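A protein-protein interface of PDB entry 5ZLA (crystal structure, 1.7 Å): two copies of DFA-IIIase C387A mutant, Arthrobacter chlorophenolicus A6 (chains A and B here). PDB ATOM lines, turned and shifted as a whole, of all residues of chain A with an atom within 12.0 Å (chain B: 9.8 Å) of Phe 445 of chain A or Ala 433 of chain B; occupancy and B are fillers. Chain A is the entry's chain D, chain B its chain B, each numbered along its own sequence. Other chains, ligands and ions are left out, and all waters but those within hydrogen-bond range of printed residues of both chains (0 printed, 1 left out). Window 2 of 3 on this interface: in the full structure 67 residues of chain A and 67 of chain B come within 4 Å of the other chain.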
ATOM      1  N   ALA A 439     -38.615  -1.022  -0.643  1.00  0.00           N
ATOM      2  CA  ALA A 439     -37.811  -0.154  -1.489  1.00  0.00           C
ATOM      3  C   ALA A 439     -36.925  -0.992  -2.394  1.00  0.00           C
ATOM      4  O   ALA A 439     -36.469  -2.066  -2.004  1.00  0.00           O
ATOM      5  CB  ALA A 439     -36.942   0.760  -0.630  1.00  0.00           C
ATOM      6  N   THR A 440     -36.680  -0.504  -3.599  1.00  0.00           N
ATOM      7  CA  THR A 440     -35.652  -1.092  -4.447  1.00  0.00           C
ATOM      8  C   THR A 440     -34.332  -1.086  -3.651  1.00  0.00           C
ATOM      9  O   THR A 440     -34.012  -0.086  -3.009  1.00  0.00           O
ATOM     10  CB  THR A 440     -35.487  -0.281  -5.746  1.00  0.00           C
ATOM     11  OG1 THR A 440     -36.743  -0.218  -6.427  1.00  0.00           O
ATOM     12  CG2 THR A 440     -34.434  -0.912  -6.664  1.00  0.00           C
ATOM     13  N   PRO A 441     -33.576  -2.205  -3.652  1.00  0.00           N
ATOM     14  CA  PRO A 441     -32.286  -2.191  -2.961  1.00  0.00           C
ATOM     15  C   PRO A 441     -31.374  -1.043  -3.413  1.00  0.00           C
ATOM     16  O   PRO A 441     -31.391  -0.658  -4.587  1.00  0.00           O
ATOM     17  CB  PRO A 441     -31.676  -3.535  -3.353  1.00  0.00           C
ATOM     18  CG  PRO A 441     -32.866  -4.425  -3.468  1.00  0.00           C
ATOM     19  CD  PRO A 441     -33.928  -3.569  -4.097  1.00  0.00           C
ATOM     20  N   THR A 442     -30.594  -0.523  -2.476  1.00  0.00           N
ATOM     21  CA  THR A 442     -29.681   0.584  -2.733  1.00  0.00           C
ATOM     22  C   THR A 442     -28.372   0.045  -3.278  1.00  0.00           C
ATOM     23  O   THR A 442     -28.038  -1.128  -3.095  1.00  0.00           O
ATOM     24  CB  THR A 442     -29.356   1.350  -1.435  1.00  0.00           C
ATOM     25  OG1 THR A 442     -28.773   0.450  -0.486  1.00  0.00           O
ATOM     26  CG2 THR A 442     -30.612   1.979  -0.838  1.00  0.00           C
ATOM     27  N   VAL A 443     -27.621   0.921  -3.931  1.00  0.00           N
ATOM     28  CA  VAL A 443     -26.265   0.607  -4.356  1.00  0.00           C
ATOM     29  C   VAL A 443     -25.426   0.272  -3.122  1.00  0.00           C
ATOM     30  O   VAL A 443     -25.576   0.908  -2.062  1.00  0.00           O
ATOM     31  CB  VAL A 443     -25.632   1.800  -5.122  1.00  0.00           C
ATOM     32  CG1 VAL A 443     -24.142   1.595  -5.341  1.00  0.00           C
ATOM     33  CG2 VAL A 443     -26.339   2.015  -6.454  1.00  0.00           C
ATOM     34  N   GLY A 444     -24.566  -0.737  -3.249  1.00  0.00           N
ATOM     35  CA  GLY A 444     -23.536  -0.996  -2.255  1.00  0.00           C
ATOM     36  C   GLY A 444     -23.880  -2.095  -1.276  1.00  0.00           C
ATOM     37  O   GLY A 444     -24.645  -3.016  -1.589  1.00  0.00           O
ATOM     38  N   PHE A 445     -23.329  -1.966  -0.071  1.00  0.00           N
ATOM     39  CA  PHE A 445     -23.402  -3.000   0.959  1.00  0.00           C
ATOM     40  C   PHE A 445     -24.453  -2.658   2.010  1.00  0.00           C
ATOM     41  O   PHE A 445     -25.362  -3.446   2.241  1.00  0.00           O
ATOM     42  CB  PHE A 445     -22.022  -3.162   1.581  1.00  0.00           C
ATOM     43  CG  PHE A 445     -20.940  -3.293   0.553  1.00  0.00           C
ATOM     44  CD1 PHE A 445     -20.757  -4.495  -0.128  1.00  0.00           C
ATOM     45  CD2 PHE A 445     -20.151  -2.192   0.195  1.00  0.00           C
ATOM     46  CE1 PHE A 445     -19.785  -4.612  -1.111  1.00  0.00           C
ATOM     47  CE2 PHE A 445     -19.177  -2.310  -0.768  1.00  0.00           C
ATOM     48  CZ  PHE A 445     -19.000  -3.515  -1.436  1.00  0.00           C
ATOM     49  N   VAL B 410     -21.478  -7.674 -15.237  1.00  0.00           N
ATOM     50  CA  VAL B 410     -21.363  -6.229 -15.362  1.00  0.00           C
ATOM     51  C   VAL B 410     -19.898  -5.870 -15.514  1.00  0.00           C
ATOM     52  O   VAL B 410     -19.128  -6.021 -14.576  1.00  0.00           O
ATOM     53  CB  VAL B 410     -21.932  -5.495 -14.129  1.00  0.00           C
ATOM     54  CG1 VAL B 410     -21.870  -3.979 -14.328  1.00  0.00           C
ATOM     55  CG2 VAL B 410     -23.360  -5.924 -13.860  1.00  0.00           C
ATOM     56  N   SER B 414     -19.546  -0.352 -16.990  1.00  0.00           N
ATOM     57  CA  SER B 414     -20.933  -0.117 -16.641  1.00  0.00           C
ATOM     58  C   SER B 414     -21.041  -0.059 -15.119  1.00  0.00           C
ATOM     59  O   SER B 414     -20.382  -0.836 -14.422  1.00  0.00           O
ATOM     60  CB  SER B 414     -21.782  -1.278 -17.184  1.00  0.00           C
ATOM     61  OG  SER B 414     -23.168  -1.051 -16.973  1.00  0.00           O
ATOM     62  N   ALA B 415     -21.845   0.859 -14.600  1.00  0.00           N
ATOM     63  CA  ALA B 415     -22.030   1.006 -13.144  1.00  0.00           C
ATOM     64  C   ALA B 415     -23.393   1.619 -12.817  1.00  0.00           C
ATOM     65  O   ALA B 415     -24.125   2.000 -13.716  1.00  0.00           O
ATOM     66  CB  ALA B 415     -20.909   1.849 -12.555  1.00  0.00           C
ATOM     67  N   ARG B 416     -23.730   1.684 -11.532  1.00  0.00           N
ATOM     68  CA  ARG B 416     -25.004   2.263 -11.055  1.00  0.00           C
ATOM     69  C   ARG B 416     -26.195   1.533 -11.665  1.00  0.00           C
ATOM     70  O   ARG B 416     -27.218   2.151 -11.996  1.00  0.00           O
ATOM     71  CB  ARG B 416     -25.066   3.779 -11.314  1.00  0.00           C
ATOM     72  CG  ARG B 416     -23.840   4.477 -10.759  1.00  0.00           C
ATOM     73  CD  ARG B 416     -23.975   5.960 -10.493  1.00  0.00           C
ATOM     74  NE  ARG B 416     -24.331   6.782 -11.641  1.00  0.00           N
ATOM     75  CZ  ARG B 416     -23.485   7.365 -12.496  1.00  0.00           C
ATOM     76  NH1 ARG B 416     -22.171   7.184 -12.430  1.00  0.00           N
ATOM     77  NH2 ARG B 416     -23.982   8.121 -13.465  1.00  0.00           N
ATOM     78  N   ASN B 417     -26.044   0.219 -11.819  1.00  0.00           N
ATOM     79  CA  ASN B 417     -27.108  -0.636 -12.319  1.00  0.00           C
ATOM     80  C   ASN B 417     -27.774  -1.261 -11.127  1.00  0.00           C
ATOM     81  O   ASN B 417     -27.221  -1.263 -10.025  1.00  0.00           O
ATOM     82  CB  ASN B 417     -26.529  -1.737 -13.210  1.00  0.00           C
ATOM     83  CG  ASN B 417     -25.736  -1.183 -14.383  1.00  0.00           C
ATOM     84  OD1 ASN B 417     -26.303  -0.530 -15.252  1.00  0.00           O
ATOM     85  ND2 ASN B 417     -24.415  -1.422 -14.403  1.00  0.00           N
ATOM     86  N   ASP B 425     -25.613 -15.180  -6.054  1.00  0.00           N
ATOM     87  CA  ASP B 425     -24.411 -14.348  -5.944  1.00  0.00           C
ATOM     88  C   ASP B 425     -23.266 -14.834  -6.823  1.00  0.00           C
ATOM     89  O   ASP B 425     -22.606 -14.019  -7.466  1.00  0.00           O
ATOM     90  CB  ASP B 425     -23.938 -14.223  -4.489  1.00  0.00           C
ATOM     91  CG  ASP B 425     -24.570 -13.059  -3.772  1.00  0.00           C
ATOM     92  OD1 ASP B 425     -24.763 -11.978  -4.384  1.00  0.00           O
ATOM     93  OD2 ASP B 425     -24.868 -13.231  -2.580  1.00  0.00           O
ATOM     94  N   ALA B 430     -20.131  -8.861 -10.717  1.00  0.00           N
ATOM     95  CA  ALA B 430     -20.356  -7.425 -10.691  1.00  0.00           C
ATOM     96  C   ALA B 430     -19.785  -6.804  -9.424  1.00  0.00           C
ATOM     97  O   ALA B 430     -19.787  -7.426  -8.351  1.00  0.00           O
ATOM     98  CB  ALA B 430     -21.850  -7.118 -10.765  1.00  0.00           C
ATOM     99  N   ASP B 431     -19.362  -5.549  -9.560  1.00  0.00           N
ATOM    100  CA  ASP B 431     -18.859  -4.742  -8.454  1.00  0.00           C
ATOM    101  C   ASP B 431     -20.006  -4.362  -7.518  1.00  0.00           C
ATOM    102  O   ASP B 431     -20.867  -3.551  -7.867  1.00  0.00           O
ATOM    103  CB  ASP B 431     -18.183  -3.495  -9.039  1.00  0.00           C
ATOM    104  CG  ASP B 431     -17.495  -2.629  -7.993  1.00  0.00           C
ATOM    105  OD1 ASP B 431     -17.658  -2.868  -6.780  1.00  0.00           O
ATOM    106  OD2 ASP B 431     -16.798  -1.678  -8.419  1.00  0.00           O
ATOM    107  N   ARG B 432     -20.028  -4.962  -6.331  1.00  0.00           N
ATOM    108  CA  ARG B 432     -21.103  -4.720  -5.359  1.00  0.00           C
ATOM    109  C   ARG B 432     -21.086  -3.303  -4.789  1.00  0.00           C
ATOM    110  O   ARG B 432     -22.113  -2.824  -4.326  1.00  0.00           O
ATOM    111  CB  ARG B 432     -21.086  -5.735  -4.208  1.00  0.00           C
ATOM    112  CG  ARG B 432     -22.012  -6.930  -4.394  1.00  0.00           C
ATOM    113  CD  ARG B 432     -21.560  -7.795  -5.543  1.00  0.00           C
ATOM    114  NE  ARG B 432     -22.335  -9.041  -5.615  1.00  0.00           N
ATOM    115  CZ  ARG B 432     -22.268  -9.919  -6.612  1.00  0.00           C
ATOM    116  NH1 ARG B 432     -21.475  -9.702  -7.663  1.00  0.00           N
ATOM    117  NH2 ARG B 432     -23.003 -11.037  -6.564  1.00  0.00           N
ATOM    118  N   ALA B 433     -19.939  -2.632  -4.838  1.00  0.00           N
ATOM    119  CA  ALA B 433     -19.829  -1.280  -4.273  1.00  0.00           C
ATOM    120  C   ALA B 433     -20.629  -0.249  -5.054  1.00  0.00           C
ATOM    121  O   ALA B 433     -21.110   0.718  -4.471  1.00  0.00           O
ATOM    122  CB  ALA B 433     -18.371  -0.844  -4.187  1.00  0.00           C
ATOM    123  N   VAL B 434     -20.757  -0.457  -6.369  1.00  0.00           N
ATOM    124  CA  VAL B 434     -21.264   0.586  -7.269  1.00  0.00           C
ATOM    125  C   VAL B 434     -22.541   0.211  -8.010  1.00  0.00           C
ATOM    126  O   VAL B 434     -23.033   1.007  -8.787  1.00  0.00           O
ATOM    127  CB  VAL B 434     -20.188   1.035  -8.295  1.00  0.00           C
ATOM    128  CG1 VAL B 434     -18.924   1.466  -7.566  1.00  0.00           C
ATOM    129  CG2 VAL B 434     -19.887  -0.067  -9.302  1.00  0.00           C
ATOM    130  N   ASN B 435     -23.056  -0.994  -7.772  1.00  0.00           N
ATOM    131  CA  ASN B 435     -24.339  -1.441  -8.300  1.00  0.00           C
ATOM    132  C   ASN B 435     -25.186  -1.923  -7.129  1.00  0.00           C
ATOM    133  O   ASN B 435     -24.649  -2.242  -6.058  1.00  0.00           O
ATOM    134  CB  ASN B 435     -24.142  -2.614  -9.262  1.00  0.00           C
ATOM    135  CG  ASN B 435     -23.280  -2.266 -10.450  1.00  0.00           C
ATOM    136  OD1 ASN B 435     -23.736  -1.622 -11.384  1.00  0.00           O
ATOM    137  ND2 ASN B 435     -22.039  -2.733 -10.443  1.00  0.00           N
ATOM    138  N   ALA B 436     -26.498  -1.989  -7.349  1.00  0.00           N
ATOM    139  CA  ALA B 436     -27.457  -2.470  -6.361  1.00  0.00           C
ATOM    140  C   ALA B 436     -27.756  -3.888  -6.760  1.00  0.00           C
ATOM    141  O   ALA B 436     -28.301  -4.096  -7.826  1.00  0.00           O
ATOM    142  CB  ALA B 436     -28.728  -1.627  -6.406  1.00  0.00           C
ATOM    143  N   ILE B 437     -27.384  -4.860  -5.935  1.00  0.00           N
ATOM    144  CA  ILE B 437     -27.503  -6.267  -6.311  1.00  0.00           C
ATOM    145  C   ILE B 437     -28.309  -7.011  -5.252  1.00  0.00           C
ATOM    146  O   ILE B 437     -28.004  -6.915  -4.064  1.00  0.00           O
ATOM    147  CB  ILE B 437     -26.113  -6.922  -6.497  1.00  0.00           C
ATOM    148  CG1 ILE B 437     -25.402  -6.300  -7.716  1.00  0.00           C
ATOM    149  CG2 ILE B 437     -26.247  -8.429  -6.697  1.00  0.00           C
ATOM    150  CD1 ILE B 437     -23.923  -6.551  -7.770  1.00  0.00           C
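Among the printed residues, pairs that only touch across the chains: Pro 441 of chain A with Ala 436 of chain B (3.4 Å), Thr 442 of chain A with Ala 436 of chain B (3.4 Å), Val 443 of chain A with Ala 433 of chain B (3.3 Å), Val 443 of chain A with Val 434 of chain B (3.4 Å), Val 443 of chain A with Asn 435 of chain B (3.7 Å), Val 443 of chain A with Ala 436 of chain B (3.7 Å), Gly 444 of chain A with Ala 433 of chain B (3.7 Å), Phe 445 of chain A with Arg 432 of chain B (3.5 Å) and Phe 445 of chain A with Ala 433 of chain B (3.6 Å).
O of Arg 432 of chain B lies close to N of Gly 444 of chain A.
O of Asn 435 of chain B sits at hydrogen-bond distance from N of Gly 444 of chain A.
No position is printed for both chains.
Ala 439 of chain A touches none of the printed residues of chain B.
Of the printed residues of chain B, Val 443 of chain A touches Ala 433 (3.3 Å), Val 434 (3.4 Å), Asn 435 (3.7 Å) and Ala 436 (3.7 Å).
Of chain B, only Arg 432 (3.1 Å), Ala 433 (3.7 Å) and Asn 435 (3.2 Å) come within 4 Å of Gly 444 of chain A.
Asn 417 of chain B touches none of the printed residues of chain A.
No residue of chain A comes within 4 Å of Asp 431 of chain B.
Of chain A, only Val 443 (3.3 Å), Gly 444 (3.7 Å) and Phe 445 (3.6 Å) come within 4 Å of Ala 433 of chain B.
Printed residues of chain A within 4 Å of Val 434 of chain B: Val 443 (3.4 Å).
Asn 435 of chain B touches just these residues of chain A: Val 443 and Gly 444.
Printed residues of chain A within 4 Å of Ala 436 of chain B: Pro 441, Thr 442 and Val 443.
The nearest residue of chain A that does not touch Ala 433 of chain B is Thr 442 of chain A (7.3 Å).
Of the 7 printed residues of chain A, 5 touch a printed residue of chain B.
Printed residues of chain A that touch a printed residue of chain B: Pro 441, Thr 442, Val 443, Gly 444 and Phe 445.
Hydrophobic or aromatic side chains of chain A within 4 Å of the printed part of chain B: Val 443 and Phe 445.
Among the printed residues, 11 pairs touch across the chains.
Among the printed residues, no Asp or Glu carboxylate lies within 4 Å of a Lys or Arg side-chain nitrogen of the other chain.
N of Arg 416 of chain B is in hydrogen-bond range of O of Val 434 of chain B.
The backbone NH of Asn 417 of chain B lies within hydrogen-bond range of the side-chain amide oxygen of Asn 435 of chain B, 3.0 Å away.
The backbone carbonyl oxygen (O) of Asn 417 of chain B lies within hydrogen-bond range of the backbone NH (N) of Ala 436 of chain B, 2.9 Å away.
The backbone carbonyl oxygen (O) of Ala 430 of chain B lies within hydrogen-bond range of the guanidinium group (NH1) of Arg 432 of chain B (2.9 Å).
The side-chain carboxylate (OD1) of Asp 431 of chain B lies within hydrogen-bond range of the backbone NH (N) of Ala 433 of chain B (3.0 Å).
The side-chain amide nitrogen of Asn 435 of chain B sits at hydrogen-bond distance from the backbone carbonyl oxygen of Asp 431 of chain B, 2.9 Å away.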
